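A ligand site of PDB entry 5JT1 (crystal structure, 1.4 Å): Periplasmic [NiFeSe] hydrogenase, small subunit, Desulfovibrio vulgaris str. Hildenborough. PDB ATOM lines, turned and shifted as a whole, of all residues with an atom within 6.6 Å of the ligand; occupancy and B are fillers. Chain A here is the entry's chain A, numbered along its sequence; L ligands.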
ATOM      1  N   ILE A 241       9.813  17.038 -12.462  1.00  0.00           N
ATOM      2  CA  ILE A 241       8.861  15.926 -12.396  1.00  0.00           C
ATOM      3  C   ILE A 241       8.127  15.923 -11.060  1.00  0.00           C
ATOM      4  O   ILE A 241       6.888  15.849 -11.015  1.00  0.00           O
ATOM      5  CB  ILE A 241       9.584  14.584 -12.623  1.00  0.00           C
ATOM      6  CG1 ILE A 241      10.071  14.476 -14.068  1.00  0.00           C
ATOM      7  CG2 ILE A 241       8.639  13.440 -12.303  1.00  0.00           C
ATOM      8  CD1 ILE A 241      10.633  13.143 -14.463  1.00  0.00           C
ATOM      9  N   HIS A 242       8.869  15.944  -9.961  1.00  0.00           N
ATOM     10  CA  HIS A 242       8.273  15.774  -8.638  1.00  0.00           C
ATOM     11  C   HIS A 242       7.244  16.860  -8.315  1.00  0.00           C
ATOM     12  O   HIS A 242       6.173  16.551  -7.774  1.00  0.00           O
ATOM     13  CB  HIS A 242       9.421  15.778  -7.641  1.00  0.00           C
ATOM     14  CG  HIS A 242       9.029  15.789  -6.197  1.00  0.00           C
ATOM     15  ND1 HIS A 242       8.623  14.648  -5.531  1.00  0.00           N
ATOM     16  CD2 HIS A 242       9.045  16.781  -5.274  1.00  0.00           C
ATOM     17  CE1 HIS A 242       8.375  14.959  -4.267  1.00  0.00           C
ATOM     18  NE2 HIS A 242       8.623  16.246  -4.084  1.00  0.00           N
ATOM     19  N   GLU A 243       7.537  18.123  -8.618  1.00  0.00           N
ATOM     20  CA  GLU A 243       6.607  19.192  -8.265  1.00  0.00           C
ATOM     21  C   GLU A 243       5.324  19.105  -9.071  1.00  0.00           C
ATOM     22  O   GLU A 243       4.338  19.740  -8.681  1.00  0.00           O
ATOM     23  CB  GLU A 243       7.247  20.572  -8.414  1.00  0.00           C
ATOM     24  CG  GLU A 243       8.455  20.796  -7.505  1.00  0.00           C
ATOM     25  CD  GLU A 243       8.139  20.710  -6.016  1.00  0.00           C
ATOM     26  OE1 GLU A 243       6.985  20.970  -5.603  1.00  0.00           O
ATOM     27  OE2 GLU A 243       9.047  20.364  -5.222  1.00  0.00           O
ATOM     28  N   CYS A 245       4.051  15.907  -9.909  1.00  0.00           N
ATOM     29  CA  CYS A 245       3.769  14.477  -9.896  1.00  0.00           C
ATOM     30  C   CYS A 245       2.399  14.206  -9.266  1.00  0.00           C
ATOM     31  O   CYS A 245       2.058  14.807  -8.240  1.00  0.00           O
ATOM     32  CB  CYS A 245       4.824  13.735  -9.066  1.00  0.00           C
ATOM     33  SG  CYS A 245       4.573  11.939  -9.008  1.00  0.00           S
ATOM     34  N   PRO A 246       1.637  13.247  -9.803  1.00  0.00           N
ATOM     35  CA  PRO A 246       0.336  12.938  -9.203  1.00  0.00           C
ATOM     36  C   PRO A 246       0.422  12.270  -7.843  1.00  0.00           C
ATOM     37  O   PRO A 246      -0.601  12.197  -7.149  1.00  0.00           O
ATOM     38  CB  PRO A 246      -0.348  12.051 -10.247  1.00  0.00           C
ATOM     39  CG  PRO A 246       0.738  11.453 -11.024  1.00  0.00           C
ATOM     40  CD  PRO A 246       1.860  12.488 -11.053  1.00  0.00           C
ATOM     41  N   TYR A 247       1.598  11.802  -7.411  1.00  0.00           N
ATOM     42  CA  TYR A 247       1.749  11.188  -6.101  1.00  0.00           C
ATOM     43  C   TYR A 247       2.334  12.163  -5.084  1.00  0.00           C
ATOM     44  O   TYR A 247       2.656  11.736  -3.959  1.00  0.00           O
ATOM     45  CB  TYR A 247       2.566   9.893  -6.194  1.00  0.00           C
ATOM     46  CG  TYR A 247       2.040   8.996  -7.308  1.00  0.00           C
ATOM     47  CD1 TYR A 247       0.788   8.402  -7.222  1.00  0.00           C
ATOM     48  CD2 TYR A 247       2.772   8.796  -8.461  1.00  0.00           C
ATOM     49  CE1 TYR A 247       0.300   7.632  -8.279  1.00  0.00           C
ATOM     50  CE2 TYR A 247       2.311   8.039  -9.485  1.00  0.00           C
ATOM     51  CZ  TYR A 247       1.075   7.458  -9.413  1.00  0.00           C
ATOM     52  OH  TYR A 247       0.675   6.716 -10.508  1.00  0.00           O
ATOM     53  N   LEU A 248       2.433  13.457  -5.439  1.00  0.00           N
ATOM     54  CA  LEU A 248       3.067  14.440  -4.565  1.00  0.00           C
ATOM     55  C   LEU A 248       2.333  14.566  -3.229  1.00  0.00           C
ATOM     56  O   LEU A 248       2.966  14.760  -2.177  1.00  0.00           O
ATOM     57  CB  LEU A 248       3.141  15.796  -5.285  1.00  0.00           C
ATOM     58  CG  LEU A 248       3.844  16.905  -4.508  1.00  0.00           C
ATOM     59  CD1 LEU A 248       5.314  16.578  -4.195  1.00  0.00           C
ATOM     60  CD2 LEU A 248       3.749  18.212  -5.301  1.00  0.00           C
ATOM     61  N   ASP A 249       1.011  14.453  -3.230  1.00  0.00           N
ATOM     62  CA  ASP A 249       0.298  14.478  -1.950  1.00  0.00           C
ATOM     63  C   ASP A 249       0.730  13.331  -1.035  1.00  0.00           C
ATOM     64  O   ASP A 249       0.856  13.524   0.170  1.00  0.00           O
ATOM     65  CB  ASP A 249      -1.217  14.537  -2.147  1.00  0.00           C
ATOM     66  CG  ASP A 249      -1.778  13.359  -2.957  1.00  0.00           C
ATOM     67  OD1 ASP A 249      -1.040  12.669  -3.710  1.00  0.00           O
ATOM     68  OD2 ASP A 249      -3.017  13.137  -2.861  1.00  0.00           O
ATOM     69  N   LYS A 250       0.946  12.138  -1.597  1.00  0.00           N
ATOM     70  CA  LYS A 250       1.427  11.008  -0.783  1.00  0.00           C
ATOM     71  C   LYS A 250       2.841  11.246  -0.252  1.00  0.00           C
ATOM     72  O   LYS A 250       3.137  10.942   0.919  1.00  0.00           O
ATOM     73  CB  LYS A 250       1.357   9.701  -1.576  1.00  0.00           C
ATOM     74  CG  LYS A 250      -0.045   9.358  -2.050  1.00  0.00           C
ATOM     75  CD  LYS A 250      -0.974   9.084  -0.879  1.00  0.00           C
ATOM     76  CE  LYS A 250      -2.372   8.795  -1.348  1.00  0.00           C
ATOM     77  NZ  LYS A 250      -3.288   8.796  -0.198  1.00  0.00           N
ATOM     78  N   TYR A 251       3.731  11.810  -1.071  1.00  0.00           N
ATOM     79  CA  TYR A 251       5.056  12.201  -0.584  1.00  0.00           C
ATOM     80  C   TYR A 251       4.941  13.126   0.624  1.00  0.00           C
ATOM     81  O   TYR A 251       5.582  12.899   1.665  1.00  0.00           O
ATOM     82  CB  TYR A 251       5.825  12.905  -1.715  1.00  0.00           C
ATOM     83  CG  TYR A 251       7.186  13.424  -1.307  1.00  0.00           C
ATOM     84  CD1 TYR A 251       8.322  12.622  -1.414  1.00  0.00           C
ATOM     85  CD2 TYR A 251       7.357  14.717  -0.821  1.00  0.00           C
ATOM     86  CE1 TYR A 251       9.576  13.098  -1.056  1.00  0.00           C
ATOM     87  CE2 TYR A 251       8.591  15.200  -0.473  1.00  0.00           C
ATOM     88  CZ  TYR A 251       9.694  14.375  -0.591  1.00  0.00           C
ATOM     89  OH  TYR A 251      10.937  14.862  -0.221  1.00  0.00           O
ATOM     90  N   ASP A 252       4.127  14.181   0.501  1.00  0.00           N
ATOM     91  CA  ASP A 252       4.004  15.142   1.584  1.00  0.00           C
ATOM     92  C   ASP A 252       3.413  14.516   2.839  1.00  0.00           C
ATOM     93  O   ASP A 252       3.734  14.949   3.953  1.00  0.00           O
ATOM     94  CB  ASP A 252       3.180  16.353   1.144  1.00  0.00           C
ATOM     95  CG  ASP A 252       3.940  17.263   0.200  1.00  0.00           C
ATOM     96  OD1 ASP A 252       5.183  17.245   0.175  1.00  0.00           O
ATOM     97  OD2 ASP A 252       3.273  17.989  -0.549  1.00  0.00           O
ATOM     98  N   MET A 256       4.447   5.969   1.685  1.00  0.00           N
ATOM     99  CA  MET A 256       5.454   5.454   0.756  1.00  0.00           C
ATOM    100  C   MET A 256       5.165   3.992   0.439  1.00  0.00           C
ATOM    101  O   MET A 256       4.994   3.187   1.352  1.00  0.00           O
ATOM    102  CB  MET A 256       6.843   5.491   1.394  1.00  0.00           C
ATOM    103  CG  MET A 256       7.344   6.867   1.697  1.00  0.00           C
ATOM    104  SD  MET A 256       7.609   7.781   0.177  1.00  0.00           S
ATOM    105  CE  MET A 256       7.986   9.402   0.870  1.00  0.00           C
ATOM    106  N   GLY A 265       0.923   4.610  -3.030  1.00  0.00           N
ATOM    107  CA  GLY A 265       1.908   5.411  -2.329  1.00  0.00           C
ATOM    108  C   GLY A 265       2.918   6.078  -3.258  1.00  0.00           C
ATOM    109  O   GLY A 265       3.030   5.783  -4.435  1.00  0.00           O
ATOM    110  N   CYS A 266       3.653   7.031  -2.675  1.00  0.00           N
ATOM    111  CA  CYS A 266       4.786   7.636  -3.373  1.00  0.00           C
ATOM    112  C   CYS A 266       5.920   6.622  -3.491  1.00  0.00           C
ATOM    113  O   CYS A 266       6.064   5.719  -2.647  1.00  0.00           O
ATOM    114  CB  CYS A 266       5.235   8.888  -2.592  1.00  0.00           C
ATOM    115  SG  CYS A 266       6.879   9.584  -2.967  1.00  0.00           S
ATOM    116  N   ARG A 267       6.691   6.733  -4.568  1.00  0.00           N
ATOM    117  CA  ARG A 267       7.773   5.810  -4.921  1.00  0.00           C
ATOM    118  C   ARG A 267       9.162   6.247  -4.411  1.00  0.00           C
ATOM    119  O   ARG A 267      10.166   5.618  -4.755  1.00  0.00           O
ATOM    120  CB  ARG A 267       7.810   5.698  -6.456  1.00  0.00           C
ATOM    121  CG  ARG A 267       6.677   4.914  -7.101  1.00  0.00           C
ATOM    122  CD  ARG A 267       5.308   5.588  -7.059  1.00  0.00           C
ATOM    123  NE  ARG A 267       4.450   5.082  -8.136  1.00  0.00           N
ATOM    124  CZ  ARG A 267       3.120   4.959  -8.102  1.00  0.00           C
ATOM    125  NH1 ARG A 267       2.415   5.281  -7.015  1.00  0.00           N
ATOM    126  NH2 ARG A 267       2.494   4.488  -9.181  1.00  0.00           N
ATOM    127  N   TYR A 268       9.223   7.288  -3.570  1.00  0.00           N
ATOM    128  CA  TYR A 268      10.513   7.801  -3.094  1.00  0.00           C
ATOM    129  C   TYR A 268      11.363   6.737  -2.392  1.00  0.00           C
ATOM    130  O   TYR A 268      12.568   6.624  -2.654  1.00  0.00           O
ATOM    131  CB  TYR A 268      10.265   8.973  -2.141  1.00  0.00           C
ATOM    132  CG  TYR A 268      11.510   9.644  -1.652  1.00  0.00           C
ATOM    133  CD1 TYR A 268      12.194  10.531  -2.448  1.00  0.00           C
ATOM    134  CD2 TYR A 268      12.004   9.372  -0.381  1.00  0.00           C
ATOM    135  CE1 TYR A 268      13.329  11.163  -2.016  1.00  0.00           C
ATOM    136  CE2 TYR A 268      13.151  10.003   0.082  1.00  0.00           C
ATOM    137  CZ  TYR A 268      13.811  10.888  -0.754  1.00  0.00           C
ATOM    138  OH  TYR A 268      14.940  11.510  -0.301  1.00  0.00           O
ATOM    139  N   ASP A 269      10.766   5.950  -1.466  1.00  0.00           N
ATOM    140  CA  ASP A 269      11.575   4.955  -0.767  1.00  0.00           C
ATOM    141  C   ASP A 269      12.049   3.837  -1.695  1.00  0.00           C
ATOM    142  O   ASP A 269      13.051   3.187  -1.387  1.00  0.00           O
ATOM    143  CB  ASP A 269      10.812   4.313   0.398  1.00  0.00           C
ATOM    144  CG  ASP A 269      10.629   5.238   1.588  1.00  0.00           C
ATOM    145  OD1 ASP A 269      11.232   6.338   1.606  1.00  0.00           O
ATOM    146  OD2 ASP A 269       9.901   4.825   2.531  1.00  0.00           O
ATOM    147  N   CYS A 272      12.744   6.547  -6.376  1.00  0.00           N
ATOM    148  CA  CYS A 272      12.369   7.544  -7.368  1.00  0.00           C
ATOM    149  C   CYS A 272      13.228   8.806  -7.277  1.00  0.00           C
ATOM    150  O   CYS A 272      13.343   9.426  -6.218  1.00  0.00           O
ATOM    151  CB  CYS A 272      10.907   7.911  -7.172  1.00  0.00           C
ATOM    152  SG  CYS A 272      10.251   9.053  -8.472  1.00  0.00           S
ATOM    153  N   LYS A 273      13.784   9.213  -8.417  1.00  0.00           N
ATOM    154  CA  LYS A 273      14.625  10.415  -8.540  1.00  0.00           C
ATOM    155  C   LYS A 273      13.877  11.608  -9.140  1.00  0.00           C
ATOM    156  O   LYS A 273      14.515  12.601  -9.527  1.00  0.00           O
ATOM    157  CB  LYS A 273      15.912  10.116  -9.339  1.00  0.00           C
ATOM    158  CG  LYS A 273      16.762   8.965  -8.776  1.00  0.00           C
ATOM    159  CD  LYS A 273      17.048   9.110  -7.286  1.00  0.00           C
ATOM    160  CE  LYS A 273      18.019   8.053  -6.739  1.00  0.00           C
ATOM    161  NZ  LYS A 273      17.688   6.700  -7.146  1.00  0.00           N
ATOM    162  N   GLY A 274      12.544  11.554  -9.189  1.00  0.00           N
ATOM    163  CA  GLY A 274      11.754  12.689  -9.628  1.00  0.00           C
ATOM    164  C   GLY A 274      12.136  14.025  -9.004  1.00  0.00           C
ATOM    165  O   GLY A 274      12.117  15.045  -9.713  1.00  0.00           O
ATOM    166  N   PRO A 275      12.460  14.079  -7.712  1.00  0.00           N
ATOM    167  CA  PRO A 275      12.799  15.377  -7.114  1.00  0.00           C
ATOM    168  C   PRO A 275      13.958  16.094  -7.772  1.00  0.00           C
ATOM    169  O   PRO A 275      14.014  17.335  -7.737  1.00  0.00           O
ATOM    170  CB  PRO A 275      13.097  15.026  -5.646  1.00  0.00           C
ATOM    171  CG  PRO A 275      12.284  13.810  -5.382  1.00  0.00           C
ATOM    172  CD  PRO A 275      12.308  13.029  -6.676  1.00  0.00           C
ATOM    173  N   TRP A 292       4.180   5.626 -17.918  1.00  0.00           N
ATOM    174  CA  TRP A 292       5.443   6.337 -17.714  1.00  0.00           C
ATOM    175  C   TRP A 292       6.144   5.758 -16.495  1.00  0.00           C
ATOM    176  O   TRP A 292       5.590   4.946 -15.755  1.00  0.00           O
ATOM    177  CB  TRP A 292       5.260   7.854 -17.580  1.00  0.00           C
ATOM    178  CG  TRP A 292       4.516   8.345 -16.351  1.00  0.00           C
ATOM    179  CD1 TRP A 292       3.241   8.029 -15.954  1.00  0.00           C
ATOM    180  CD2 TRP A 292       5.014   9.301 -15.403  1.00  0.00           C
ATOM    181  NE1 TRP A 292       2.935   8.726 -14.813  1.00  0.00           N
ATOM    182  CE2 TRP A 292       4.005   9.503 -14.442  1.00  0.00           C
ATOM    183  CE3 TRP A 292       6.223  10.004 -15.279  1.00  0.00           C
ATOM    184  CZ2 TRP A 292       4.148  10.408 -13.380  1.00  0.00           C
ATOM    185  CZ3 TRP A 292       6.372  10.904 -14.223  1.00  0.00           C
ATOM    186  CH2 TRP A 292       5.330  11.099 -13.288  1.00  0.00           C
ATOM    187  N   VAL A 294       7.291   6.652 -13.526  1.00  0.00           N
ATOM    188  CA  VAL A 294       6.864   6.776 -12.136  1.00  0.00           C
ATOM    189  C   VAL A 294       5.628   5.944 -11.835  1.00  0.00           C
ATOM    190  O   VAL A 294       5.517   5.335 -10.774  1.00  0.00           O
ATOM    191  CB  VAL A 294       6.660   8.261 -11.760  1.00  0.00           C
ATOM    192  CG1 VAL A 294       6.003   8.403 -10.363  1.00  0.00           C
ATOM    193  CG2 VAL A 294       7.997   9.006 -11.798  1.00  0.00           C
ATOM    194  N   ALA A 297       7.126   2.076 -12.152  1.00  0.00           N
ATOM    195  CA  ALA A 297       8.182   1.681 -11.233  1.00  0.00           C
ATOM    196  C   ALA A 297       8.726   2.934 -10.559  1.00  0.00           C
ATOM    197  O   ALA A 297       8.059   3.464  -9.657  1.00  0.00           O
ATOM    198  CB  ALA A 297       9.290   0.914 -11.970  1.00  0.00           C
ATOM    199  N   CYS A 299      11.250   6.772 -11.406  1.00  0.00           N
ATOM    200  CA  CYS A 299      12.109   7.586 -12.265  1.00  0.00           C
ATOM    201  C   CYS A 299      13.570   7.376 -11.868  1.00  0.00           C
ATOM    202  O   CYS A 299      13.908   7.355 -10.676  1.00  0.00           O
ATOM    203  CB  CYS A 299      11.743   9.063 -12.142  1.00  0.00           C
ATOM    204  SG  CYS A 299      12.786  10.268 -13.073  1.00  0.00           S
HETATM  205 FE1  LIG L   1       8.681  10.275  -7.300  1.00  0.00          FE
HETATM  206 FE2  LIG L   1       8.164  12.732  -6.157  1.00  0.00          FE
HETATM  207 FE3  LIG L   1       7.035  10.524  -5.071  1.00  0.00          FE
HETATM  208 FE4  LIG L   1       6.231  11.445  -7.505  1.00  0.00          FE
HETATM  209  S1  LIG L   1       5.963  12.472  -5.488  1.00  0.00           S
HETATM  210  S2  LIG L   1       6.602   9.262  -6.916  1.00  0.00           S
HETATM  211  S3  LIG L   1       8.232  12.243  -8.390  1.00  0.00           S
HETATM  212  S4  LIG L   1       9.308  10.970  -5.201  1.00  0.00           S
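An iron atom (FE2) of the ligand is bound by a ring nitrogen (ND1) of His 242, at 2.1 Å.
FE4 of the ligand is bound by SG of Cys 245 (2.3 Å).
SG of Cys 272 binds FE1 of the ligand (2.3 Å).
SG of Cys 266 is bound to FE3 of the ligand, at 2.3 Å.
A sulfur (S2) of the ligand lies close to the backbone NH of Arg 267 (3.5 Å).
S1 of the ligand lies close to N of Leu 248 (3.7 Å).
The backbone NH (N) of His 242 sits at hydrogen-bond distance from the backbone carbonyl oxygen (O) of Gly 274, at 3.4 Å.
The backbone NH of Tyr 247 sits close to the side-chain sulfur of Cys 245 (3.4 Å).
N of Cys 272 is in hydrogen-bond range of O of Arg 267, 3.2 Å away.
The side-chain sulfur (SG) of Cys 272 lies close to the backbone NH (N) of Gly 274 (3.5 Å).
SG of Cys 266 lies close to N of Tyr 268, at 3.3 Å.
The side-chain sulfur (SG) of Cys 266 lies close to the side-chain sulfur (SD) of Met 256 (3.7 Å).
The guanidinium group of Arg 267 sits at hydrogen-bond distance from the backbone carbonyl oxygen of Val 294 (2.9 Å).
OH of Tyr 247 is in hydrogen-bond range of NH2 of Arg 267 (3.2 Å).
O of Tyr 247 sits close to S1 of the ligand (3.7 Å).
Tyr 251 touches the ligand (CB to S1, 3.8 Å).
CB of Tyr 268 touches S4 of the ligand, 3.8 Å away.
Gly 274 touches the ligand.
Pro 275 touches the ligand.
CG1 of Val 294 touches S2 of the ligand, 3.6 Å away.
Hydrophobic or aromatic side chains that line the ligand: His 242, Tyr 251, Tyr 268, Pro 275 and Val 294.
12 residues have an atom within 4 Å of the ligand: His 242, Cys 245, Tyr 247, Leu 248, Tyr 251, Cys 266, Arg 267, Tyr 268, Cys 272, Gly 274, Pro 275 and Val 294.
The nearest printed residue that does not touch the ligand is Ile 241 (4.1 Å).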
